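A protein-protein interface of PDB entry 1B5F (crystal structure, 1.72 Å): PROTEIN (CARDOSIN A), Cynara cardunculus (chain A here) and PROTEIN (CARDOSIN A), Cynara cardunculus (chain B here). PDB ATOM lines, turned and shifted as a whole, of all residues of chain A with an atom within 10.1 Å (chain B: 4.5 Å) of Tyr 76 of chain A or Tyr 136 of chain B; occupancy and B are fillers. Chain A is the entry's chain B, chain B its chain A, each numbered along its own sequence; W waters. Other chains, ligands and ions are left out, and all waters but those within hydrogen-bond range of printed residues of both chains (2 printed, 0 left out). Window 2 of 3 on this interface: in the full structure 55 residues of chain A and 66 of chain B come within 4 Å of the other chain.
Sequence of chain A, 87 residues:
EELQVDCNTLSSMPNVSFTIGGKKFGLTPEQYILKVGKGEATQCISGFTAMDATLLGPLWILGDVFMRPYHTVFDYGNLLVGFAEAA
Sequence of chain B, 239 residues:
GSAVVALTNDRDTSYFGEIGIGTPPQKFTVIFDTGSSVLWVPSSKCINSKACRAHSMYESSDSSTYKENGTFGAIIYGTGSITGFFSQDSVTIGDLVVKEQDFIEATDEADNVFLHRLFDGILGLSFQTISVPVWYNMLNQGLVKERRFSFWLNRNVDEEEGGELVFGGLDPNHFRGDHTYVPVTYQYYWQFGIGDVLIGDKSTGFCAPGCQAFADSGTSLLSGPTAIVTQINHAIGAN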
ATOM      1  N   VAL A  73      17.563  13.032  -1.305  1.00  0.00           N
ATOM      2  CA  VAL A  73      18.730  12.289  -1.726  1.00  0.00           C
ATOM      3  C   VAL A  73      19.109  11.260  -0.667  1.00  0.00           C
ATOM      4  O   VAL A  73      19.259  11.617   0.499  1.00  0.00           O
ATOM      5  CB  VAL A  73      19.924  13.201  -1.973  1.00  0.00           C
ATOM      6  CG1 VAL A  73      21.175  12.363  -2.178  1.00  0.00           C
ATOM      7  CG2 VAL A  73      19.651  14.078  -3.186  1.00  0.00           C
ATOM      8  N   PHE A  74      19.237  10.018  -1.111  1.00  0.00           N
ATOM      9  CA  PHE A  74      19.711   8.948  -0.236  1.00  0.00           C
ATOM     10  C   PHE A  74      21.161   8.647  -0.635  1.00  0.00           C
ATOM     11  O   PHE A  74      21.395   8.048  -1.676  1.00  0.00           O
ATOM     12  CB  PHE A  74      18.827   7.709  -0.328  1.00  0.00           C
ATOM     13  CG  PHE A  74      17.387   8.020   0.059  1.00  0.00           C
ATOM     14  CD1 PHE A  74      16.502   8.562  -0.850  1.00  0.00           C
ATOM     15  CD2 PHE A  74      16.986   7.752   1.361  1.00  0.00           C
ATOM     16  CE1 PHE A  74      15.195   8.857  -0.431  1.00  0.00           C
ATOM     17  CE2 PHE A  74      15.697   8.051   1.778  1.00  0.00           C
ATOM     18  CZ  PHE A  74      14.811   8.620   0.869  1.00  0.00           C
ATOM     19  N   ASP A  75      22.068   9.096   0.211  1.00  0.00           N
ATOM     20  CA  ASP A  75      23.509   8.981  -0.038  1.00  0.00           C
ATOM     21  C   ASP A  75      24.050   7.759   0.689  1.00  0.00           C
ATOM     22  O   ASP A  75      24.377   7.830   1.856  1.00  0.00           O
ATOM     23  CB  ASP A  75      24.236  10.250   0.374  1.00  0.00           C
ATOM     24  CG  ASP A  75      25.716  10.236   0.014  1.00  0.00           C
ATOM     25  OD1 ASP A  75      26.258   9.157  -0.292  1.00  0.00           O
ATOM     26  OD2 ASP A  75      26.348  11.306   0.059  1.00  0.00           O
ATOM     27  N   TYR A  76      24.121   6.644  -0.041  1.00  0.00           N
ATOM     28  CA  TYR A  76      24.642   5.425   0.575  1.00  0.00           C
ATOM     29  C   TYR A  76      26.145   5.484   0.827  1.00  0.00           C
ATOM     30  O   TYR A  76      26.676   5.047   1.857  1.00  0.00           O
ATOM     31  CB  TYR A  76      24.276   4.269  -0.356  1.00  0.00           C
ATOM     32  CG  TYR A  76      24.627   2.921   0.222  1.00  0.00           C
ATOM     33  CD1 TYR A  76      23.773   2.286   1.107  1.00  0.00           C
ATOM     34  CD2 TYR A  76      25.821   2.306  -0.125  1.00  0.00           C
ATOM     35  CE1 TYR A  76      24.087   1.054   1.645  1.00  0.00           C
ATOM     36  CE2 TYR A  76      26.150   1.073   0.400  1.00  0.00           C
ATOM     37  CZ  TYR A  76      25.283   0.462   1.278  1.00  0.00           C
ATOM     38  OH  TYR A  76      25.621  -0.774   1.799  1.00  0.00           O
ATOM     39  N   GLY A  77      26.908   6.028  -0.116  1.00  0.00           N
ATOM     40  CA  GLY A  77      28.348   6.097   0.017  1.00  0.00           C
ATOM     41  C   GLY A  77      28.793   6.825   1.265  1.00  0.00           C
ATOM     42  O   GLY A  77      29.801   6.448   1.873  1.00  0.00           O
ATOM     43  N   ASN A  78      28.080   7.861   1.698  1.00  0.00           N
ATOM     44  CA  ASN A  78      28.415   8.611   2.887  1.00  0.00           C
ATOM     45  C   ASN A  78      27.450   8.426   4.054  1.00  0.00           C
ATOM     46  O   ASN A  78      27.644   9.009   5.136  1.00  0.00           O
ATOM     47  CB  ASN A  78      28.394  10.117   2.556  1.00  0.00           C
ATOM     48  CG  ASN A  78      29.450  10.516   1.544  1.00  0.00           C
ATOM     49  OD1 ASN A  78      29.154  11.109   0.514  1.00  0.00           O
ATOM     50  ND2 ASN A  78      30.694  10.178   1.837  1.00  0.00           N
ATOM     51  N   LEU A  79      26.413   7.639   3.830  1.00  0.00           N
ATOM     52  CA  LEU A  79      25.371   7.424   4.827  1.00  0.00           C
ATOM     53  C   LEU A  79      24.746   8.752   5.297  1.00  0.00           C
ATOM     54  O   LEU A  79      24.737   9.073   6.484  1.00  0.00           O
ATOM     55  CB  LEU A  79      25.877   6.690   6.052  1.00  0.00           C
ATOM     56  CG  LEU A  79      25.631   5.197   6.241  1.00  0.00           C
ATOM     57  CD1 LEU A  79      24.943   4.955   7.574  1.00  0.00           C
ATOM     58  CD2 LEU A  79      24.850   4.589   5.094  1.00  0.00           C
ATOM     59  N   LEU A  80      24.213   9.513   4.344  1.00  0.00           N
ATOM     60  CA  LEU A  80      23.552  10.783   4.572  1.00  0.00           C
ATOM     61  C   LEU A  80      22.163  10.786   3.925  1.00  0.00           C
ATOM     62  O   LEU A  80      22.007  10.083   2.924  1.00  0.00           O
ATOM     63  CB  LEU A  80      24.340  11.919   3.937  1.00  0.00           C
ATOM     64  CG  LEU A  80      25.810  12.075   4.298  1.00  0.00           C
ATOM     65  CD1 LEU A  80      26.403  13.157   3.396  1.00  0.00           C
ATOM     66  CD2 LEU A  80      26.028  12.409   5.747  1.00  0.00           C
ATOM     67  N   VAL A  81      21.278  11.591   4.475  1.00  0.00           N
ATOM     68  CA  VAL A  81      20.000  11.919   3.841  1.00  0.00           C
ATOM     69  C   VAL A  81      19.993  13.438   3.593  1.00  0.00           C
ATOM     70  O   VAL A  81      20.352  14.186   4.491  1.00  0.00           O
ATOM     71  CB  VAL A  81      18.786  11.515   4.671  1.00  0.00           C
ATOM     72  CG1 VAL A  81      17.487  11.868   3.962  1.00  0.00           C
ATOM     73  CG2 VAL A  81      18.776  10.016   4.939  1.00  0.00           C
ATOM     74  N   GLY A  82      19.609  13.865   2.402  1.00  0.00           N
ATOM     75  CA  GLY A  82      19.573  15.260   2.038  1.00  0.00           C
ATOM     76  C   GLY A  82      18.208  15.694   1.556  1.00  0.00           C
ATOM     77  O   GLY A  82      17.535  14.935   0.855  1.00  0.00           O
ATOM     78  N   SER B 126      15.643   0.275   1.843  1.00  0.00           N
ATOM     79  CA  SER B 126      16.293   0.465   3.130  1.00  0.00           C
ATOM     80  C   SER B 126      17.455  -0.503   3.309  1.00  0.00           C
ATOM     81  O   SER B 126      17.776  -1.240   2.371  1.00  0.00           O
ATOM     82  CB  SER B 126      15.300   0.332   4.291  1.00  0.00           C
ATOM     83  OG  SER B 126      14.890  -1.004   4.503  1.00  0.00           O
ATOM     84  N   PHE B 127      18.079  -0.490   4.483  1.00  0.00           N
ATOM     85  CA  PHE B 127      19.311  -1.249   4.704  1.00  0.00           C
ATOM     86  C   PHE B 127      19.061  -2.739   4.863  1.00  0.00           C
ATOM     87  O   PHE B 127      18.007  -3.226   5.247  1.00  0.00           O
ATOM     88  CB  PHE B 127      20.068  -0.695   5.923  1.00  0.00           C
ATOM     89  CG  PHE B 127      20.491   0.745   5.665  1.00  0.00           C
ATOM     90  CD1 PHE B 127      21.512   1.024   4.772  1.00  0.00           C
ATOM     91  CD2 PHE B 127      19.849   1.798   6.295  1.00  0.00           C
ATOM     92  CE1 PHE B 127      21.869   2.334   4.515  1.00  0.00           C
ATOM     93  CE2 PHE B 127      20.219   3.119   6.062  1.00  0.00           C
ATOM     94  CZ  PHE B 127      21.234   3.372   5.161  1.00  0.00           C
ATOM     95  N   GLN B 128      20.072  -3.526   4.529  1.00  0.00           N
ATOM     96  CA  GLN B 128      19.923  -4.975   4.448  1.00  0.00           C
ATOM     97  C   GLN B 128      19.439  -5.603   5.742  1.00  0.00           C
ATOM     98  O   GLN B 128      19.936  -5.242   6.806  1.00  0.00           O
ATOM     99  CB  GLN B 128      21.287  -5.564   4.047  1.00  0.00           C
ATOM    100  CG  GLN B 128      21.313  -7.067   4.098  1.00  0.00           C
ATOM    101  CD  GLN B 128      22.432  -7.710   3.301  1.00  0.00           C
ATOM    102  OE1 GLN B 128      23.050  -7.135   2.408  1.00  0.00           O
ATOM    103  NE2 GLN B 128      22.589  -8.972   3.691  1.00  0.00           N
ATOM    104  N   VAL B 132      20.264  -9.581   0.288  1.00  0.00           N
ATOM    105  CA  VAL B 132      20.982  -8.414  -0.245  1.00  0.00           C
ATOM    106  C   VAL B 132      20.024  -7.589  -1.096  1.00  0.00           C
ATOM    107  O   VAL B 132      19.546  -8.117  -2.112  1.00  0.00           O
ATOM    108  CB  VAL B 132      22.225  -8.831  -1.032  1.00  0.00           C
ATOM    109  CG1 VAL B 132      22.950  -7.621  -1.609  1.00  0.00           C
ATOM    110  CG2 VAL B 132      23.159  -9.638  -0.133  1.00  0.00           C
ATOM    111  N   PRO B 133      19.715  -6.358  -0.731  1.00  0.00           N
ATOM    112  CA  PRO B 133      18.790  -5.548  -1.537  1.00  0.00           C
ATOM    113  C   PRO B 133      19.317  -5.173  -2.911  1.00  0.00           C
ATOM    114  O   PRO B 133      20.508  -5.170  -3.211  1.00  0.00           O
ATOM    115  CB  PRO B 133      18.628  -4.244  -0.720  1.00  0.00           C
ATOM    116  CG  PRO B 133      19.046  -4.626   0.653  1.00  0.00           C
ATOM    117  CD  PRO B 133      20.163  -5.616   0.466  1.00  0.00           C
ATOM    118  N   VAL B 134      18.388  -4.817  -3.785  1.00  0.00           N
ATOM    119  CA  VAL B 134      18.640  -4.448  -5.171  1.00  0.00           C
ATOM    120  C   VAL B 134      19.726  -3.377  -5.264  1.00  0.00           C
ATOM    121  O   VAL B 134      20.640  -3.444  -6.087  1.00  0.00           O
ATOM    122  CB  VAL B 134      17.356  -3.915  -5.834  1.00  0.00           C
ATOM    123  CG1 VAL B 134      17.652  -3.198  -7.132  1.00  0.00           C
ATOM    124  CG2 VAL B 134      16.388  -5.070  -6.053  1.00  0.00           C
ATOM    125  N   TRP B 135      19.594  -2.371  -4.405  1.00  0.00           N
ATOM    126  CA  TRP B 135      20.531  -1.253  -4.441  1.00  0.00           C
ATOM    127  C   TRP B 135      21.960  -1.700  -4.152  1.00  0.00           C
ATOM    128  O   TRP B 135      22.883  -1.241  -4.833  1.00  0.00           O
ATOM    129  CB  TRP B 135      20.099  -0.179  -3.441  1.00  0.00           C
ATOM    130  CG  TRP B 135      21.185   0.841  -3.209  1.00  0.00           C
ATOM    131  CD1 TRP B 135      21.900   1.034  -2.064  1.00  0.00           C
ATOM    132  CD2 TRP B 135      21.670   1.803  -4.156  1.00  0.00           C
ATOM    133  NE1 TRP B 135      22.806   2.067  -2.241  1.00  0.00           N
ATOM    134  CE2 TRP B 135      22.677   2.547  -3.515  1.00  0.00           C
ATOM    135  CE3 TRP B 135      21.347   2.106  -5.477  1.00  0.00           C
ATOM    136  CZ2 TRP B 135      23.371   3.574  -4.150  1.00  0.00           C
ATOM    137  CZ3 TRP B 135      22.037   3.133  -6.111  1.00  0.00           C
ATOM    138  CH2 TRP B 135      23.036   3.849  -5.438  1.00  0.00           C
ATOM    139  N   TYR B 136      22.158  -2.572  -3.168  1.00  0.00           N
ATOM    140  CA  TYR B 136      23.482  -3.075  -2.831  1.00  0.00           C
ATOM    141  C   TYR B 136      24.063  -3.903  -3.985  1.00  0.00           C
ATOM    142  O   TYR B 136      25.268  -3.841  -4.290  1.00  0.00           O
ATOM    143  CB  TYR B 136      23.448  -3.937  -1.600  1.00  0.00           C
ATOM    144  CG  TYR B 136      23.193  -3.426  -0.220  1.00  0.00           C
ATOM    145  CD1 TYR B 136      22.154  -2.538   0.057  1.00  0.00           C
ATOM    146  CD2 TYR B 136      23.975  -3.843   0.851  1.00  0.00           C
ATOM    147  CE1 TYR B 136      21.925  -2.077   1.331  1.00  0.00           C
ATOM    148  CE2 TYR B 136      23.745  -3.394   2.134  1.00  0.00           C
ATOM    149  CZ  TYR B 136      22.713  -2.505   2.373  1.00  0.00           C
ATOM    150  OH  TYR B 136      22.454  -2.046   3.646  1.00  0.00           O
ATOM    151  N   ASN B 137      23.211  -4.702  -4.634  1.00  0.00           N
ATOM    152  CA  ASN B 137      23.693  -5.461  -5.791  1.00  0.00           C
ATOM    153  C   ASN B 137      24.064  -4.517  -6.929  1.00  0.00           C
ATOM    154  O   ASN B 137      25.030  -4.703  -7.669  1.00  0.00           O
ATOM    155  CB  ASN B 137      22.674  -6.511  -6.259  1.00  0.00           C
ATOM    156  CG  ASN B 137      22.720  -7.723  -5.336  1.00  0.00           C
ATOM    157  OD1 ASN B 137      23.802  -8.133  -4.919  1.00  0.00           O
ATOM    158  ND2 ASN B 137      21.542  -8.228  -5.006  1.00  0.00           N
ATOM    159  N   MET B 138      23.286  -3.454  -7.111  1.00  0.00           N
ATOM    160  CA  MET B 138      23.636  -2.439  -8.092  1.00  0.00           C
ATOM    161  C   MET B 138      25.054  -1.919  -7.899  1.00  0.00           C
ATOM    162  O   MET B 138      25.861  -1.852  -8.815  1.00  0.00           O
ATOM    163  CB  MET B 138      22.715  -1.225  -7.939  1.00  0.00           C
ATOM    164  CG  MET B 138      21.473  -1.279  -8.787  1.00  0.00           C
ATOM    165  SD  MET B 138      20.518   0.258  -8.609  1.00  0.00           S
ATOM    166  CE  MET B 138      19.113  -0.205  -9.625  1.00  0.00           C
ATOM    167  N   LEU B 139      25.301  -1.531  -6.652  1.00  0.00           N
ATOM    168  CA  LEU B 139      26.600  -0.988  -6.304  1.00  0.00           C
ATOM    169  C   LEU B 139      27.683  -2.040  -6.508  1.00  0.00           C
ATOM    170  O   LEU B 139      28.679  -1.740  -7.153  1.00  0.00           O
ATOM    171  CB  LEU B 139      26.624  -0.517  -4.853  1.00  0.00           C
ATOM    172  CG  LEU B 139      25.612   0.602  -4.553  1.00  0.00           C
ATOM    173  CD1 LEU B 139      25.527   0.859  -3.062  1.00  0.00           C
ATOM    174  CD2 LEU B 139      25.958   1.875  -5.297  1.00  0.00           C
ATOM    175  N   ASN B 140      27.432  -3.212  -5.952  1.00  0.00           N
ATOM    176  CA  ASN B 140      28.357  -4.336  -6.057  1.00  0.00           C
ATOM    177  C   ASN B 140      28.717  -4.618  -7.500  1.00  0.00           C
ATOM    178  O   ASN B 140      29.857  -4.945  -7.815  1.00  0.00           O
ATOM    179  CB  ASN B 140      27.736  -5.577  -5.406  1.00  0.00           C
ATOM    180  CG  ASN B 140      28.741  -6.693  -5.225  1.00  0.00           C
ATOM    181  OD1 ASN B 140      28.544  -7.791  -5.757  1.00  0.00           O
ATOM    182  ND2 ASN B 140      29.814  -6.459  -4.470  1.00  0.00           N
ATOM    183  N   ARG B 147      27.107   6.532  -5.570  1.00  0.00           N
ATOM    184  CA  ARG B 147      26.495   5.686  -4.561  1.00  0.00           C
ATOM    185  C   ARG B 147      25.351   6.449  -3.908  1.00  0.00           C
ATOM    186  O   ARG B 147      25.245   6.579  -2.697  1.00  0.00           O
ATOM    187  CB  ARG B 147      27.585   5.230  -3.584  1.00  0.00           C
ATOM    188  CG  ARG B 147      28.683   4.442  -4.282  1.00  0.00           C
ATOM    189  CD  ARG B 147      29.869   3.952  -3.509  1.00  0.00           C
ATOM    190  NE  ARG B 147      29.741   3.644  -2.117  1.00  0.00           N
ATOM    191  CZ  ARG B 147      29.657   2.498  -1.465  1.00  0.00           C
ATOM    192  NH1 ARG B 147      29.681   1.331  -2.102  1.00  0.00           N
ATOM    193  NH2 ARG B 147      29.546   2.520  -0.130  1.00  0.00           N
ATOM    194  N   ARG B 148      24.453   6.971  -4.746  1.00  0.00           N
ATOM    195  CA  ARG B 148      23.318   7.744  -4.259  1.00  0.00           C
ATOM    196  C   ARG B 148      22.098   7.493  -5.140  1.00  0.00           C
ATOM    197  O   ARG B 148      22.258   7.188  -6.325  1.00  0.00           O
ATOM    198  CB  ARG B 148      23.606   9.250  -4.254  1.00  0.00           C
ATOM    199  CG  ARG B 148      24.894   9.702  -3.615  1.00  0.00           C
ATOM    200  CD  ARG B 148      24.866  11.215  -3.418  1.00  0.00           C
ATOM    201  NE  ARG B 148      24.948  11.920  -4.697  1.00  0.00           N
ATOM    202  CZ  ARG B 148      25.043  13.256  -4.730  1.00  0.00           C
ATOM    203  NH1 ARG B 148      25.057  13.976  -3.630  1.00  0.00           N
ATOM    204  NH2 ARG B 148      25.116  13.872  -5.885  1.00  0.00           N
ATOM    205  N   TRP B 190      16.272   4.755   6.682  1.00  0.00           N
ATOM    206  CA  TRP B 190      17.141   5.895   6.427  1.00  0.00           C
ATOM    207  C   TRP B 190      16.752   6.973   7.429  1.00  0.00           C
ATOM    208  O   TRP B 190      15.996   7.896   7.160  1.00  0.00           O
ATOM    209  CB  TRP B 190      17.013   6.368   4.993  1.00  0.00           C
ATOM    210  CG  TRP B 190      17.546   5.462   3.952  1.00  0.00           C
ATOM    211  CD1 TRP B 190      16.981   4.369   3.371  1.00  0.00           C
ATOM    212  CD2 TRP B 190      18.844   5.614   3.361  1.00  0.00           C
ATOM    213  NE1 TRP B 190      17.857   3.838   2.448  1.00  0.00           N
ATOM    214  CE2 TRP B 190      18.999   4.585   2.423  1.00  0.00           C
ATOM    215  CE3 TRP B 190      19.858   6.553   3.564  1.00  0.00           C
ATOM    216  CZ2 TRP B 190      20.155   4.447   1.664  1.00  0.00           C
ATOM    217  CZ3 TRP B 190      21.000   6.398   2.797  1.00  0.00           C
ATOM    218  CH2 TRP B 190      21.139   5.374   1.875  1.00  0.00           C
HETATM  219  O   HOH W   1      25.533  13.597  -0.686  1.00  0.00           O
HETATM  220  O   HOH W   2      28.212   3.261   2.830  1.00  0.00           O
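Arg 148 of chain B touches Phe 74 of chain A (CA to O, 3.2 Å). Asp 75 of chain A touches Arg 148 of chain B. Asp 75 of chain A touches Trp 190 of chain B. Trp 135 of chain B touches Tyr 76 of chain A (NE1 to CG, 3.2 Å). Tyr 76 of chain A touches Tyr 136 of chain B (OH to CE2, 3.2 Å). CD1 of Leu 139 of chain B touches CD2 of Tyr 76 of chain A, 3.3 Å away. Trp 190 of chain B touches Tyr 76 of chain A. Leu 79 of chain A touches Phe 127 of chain B. Leu 80 of chain A touches Trp 190 of chain B. Val 81 of chain A touches Trp 190 of chain B (CG2 to CE3, 3.9 Å).
The side-chain carboxylate (OD2) of Asp 75 of chain A sits close to the side-chain amide oxygen (OD1) of Asn 78 of chain A (2.8 Å). The backbone NH (N) of Asp 75 of chain A lies within hydrogen-bond range of the backbone carbonyl oxygen (O) of Leu 80 of chain A (2.9 Å). The side-chain carboxylate (OD1) of Asp 75 of chain A is in hydrogen-bond range of the backbone NH (N) of Gly 77 of chain A (3.2 Å). The side-chain hydroxyl (OH) of Tyr 136 of chain B lies within hydrogen-bond range of the backbone NH (N) of Gln 128 of chain B (2.9 Å).
Tyr 76 of chain A touches just these residues of chain B: Phe 127, Trp 135, Tyr 136, Leu 139, Arg 147 and Trp 190. Tyr 136 of chain B touches one residue of chain A. No residue of chain A comes within 4 Å of Pro 133 of chain B. No residue of chain A comes within 4 Å of Asn 140 of chain B. Of the printed residues of chain A, Arg 148 of chain B touches Phe 74 and Asp 75. Of the printed residues of chain B, Asp 75 of chain A touches Arg 147 (3.7 Å), Arg 148 (3.6 Å) and Trp 190 (3.8 Å).
Printed residues of chain A that touch a printed residue of chain B: Phe 74, Asp 75, Tyr 76, Gly 77, Leu 79, Leu 80 and Val 81. Hydrophobic or aromatic side chains of chain A within 4 Å of the printed part of chain B: Phe 74, Tyr 76, Leu 79 and Val 81. Among the printed residues, 15 pairs touch across the chains.
Water W1 bridges OD2 of Asp 75 of chain A and NH1 of Arg 148 of chain B. Water W2 lies within hydrogen-bond range of O of Tyr 76 of chain A (2.5 Å) and NH2 of Arg 147 of chain B (3.3 Å).
The backbone carbonyl oxygen (O) of Arg 147 of chain B sits at hydrogen-bond distance from the backbone NH (N) of Tyr 76 of chain A (2.9 Å). The backbone carbonyl oxygen of Arg 147 of chain B lies within hydrogen-bond range of the backbone NH of Gly 77 of chain A (3.1 Å).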
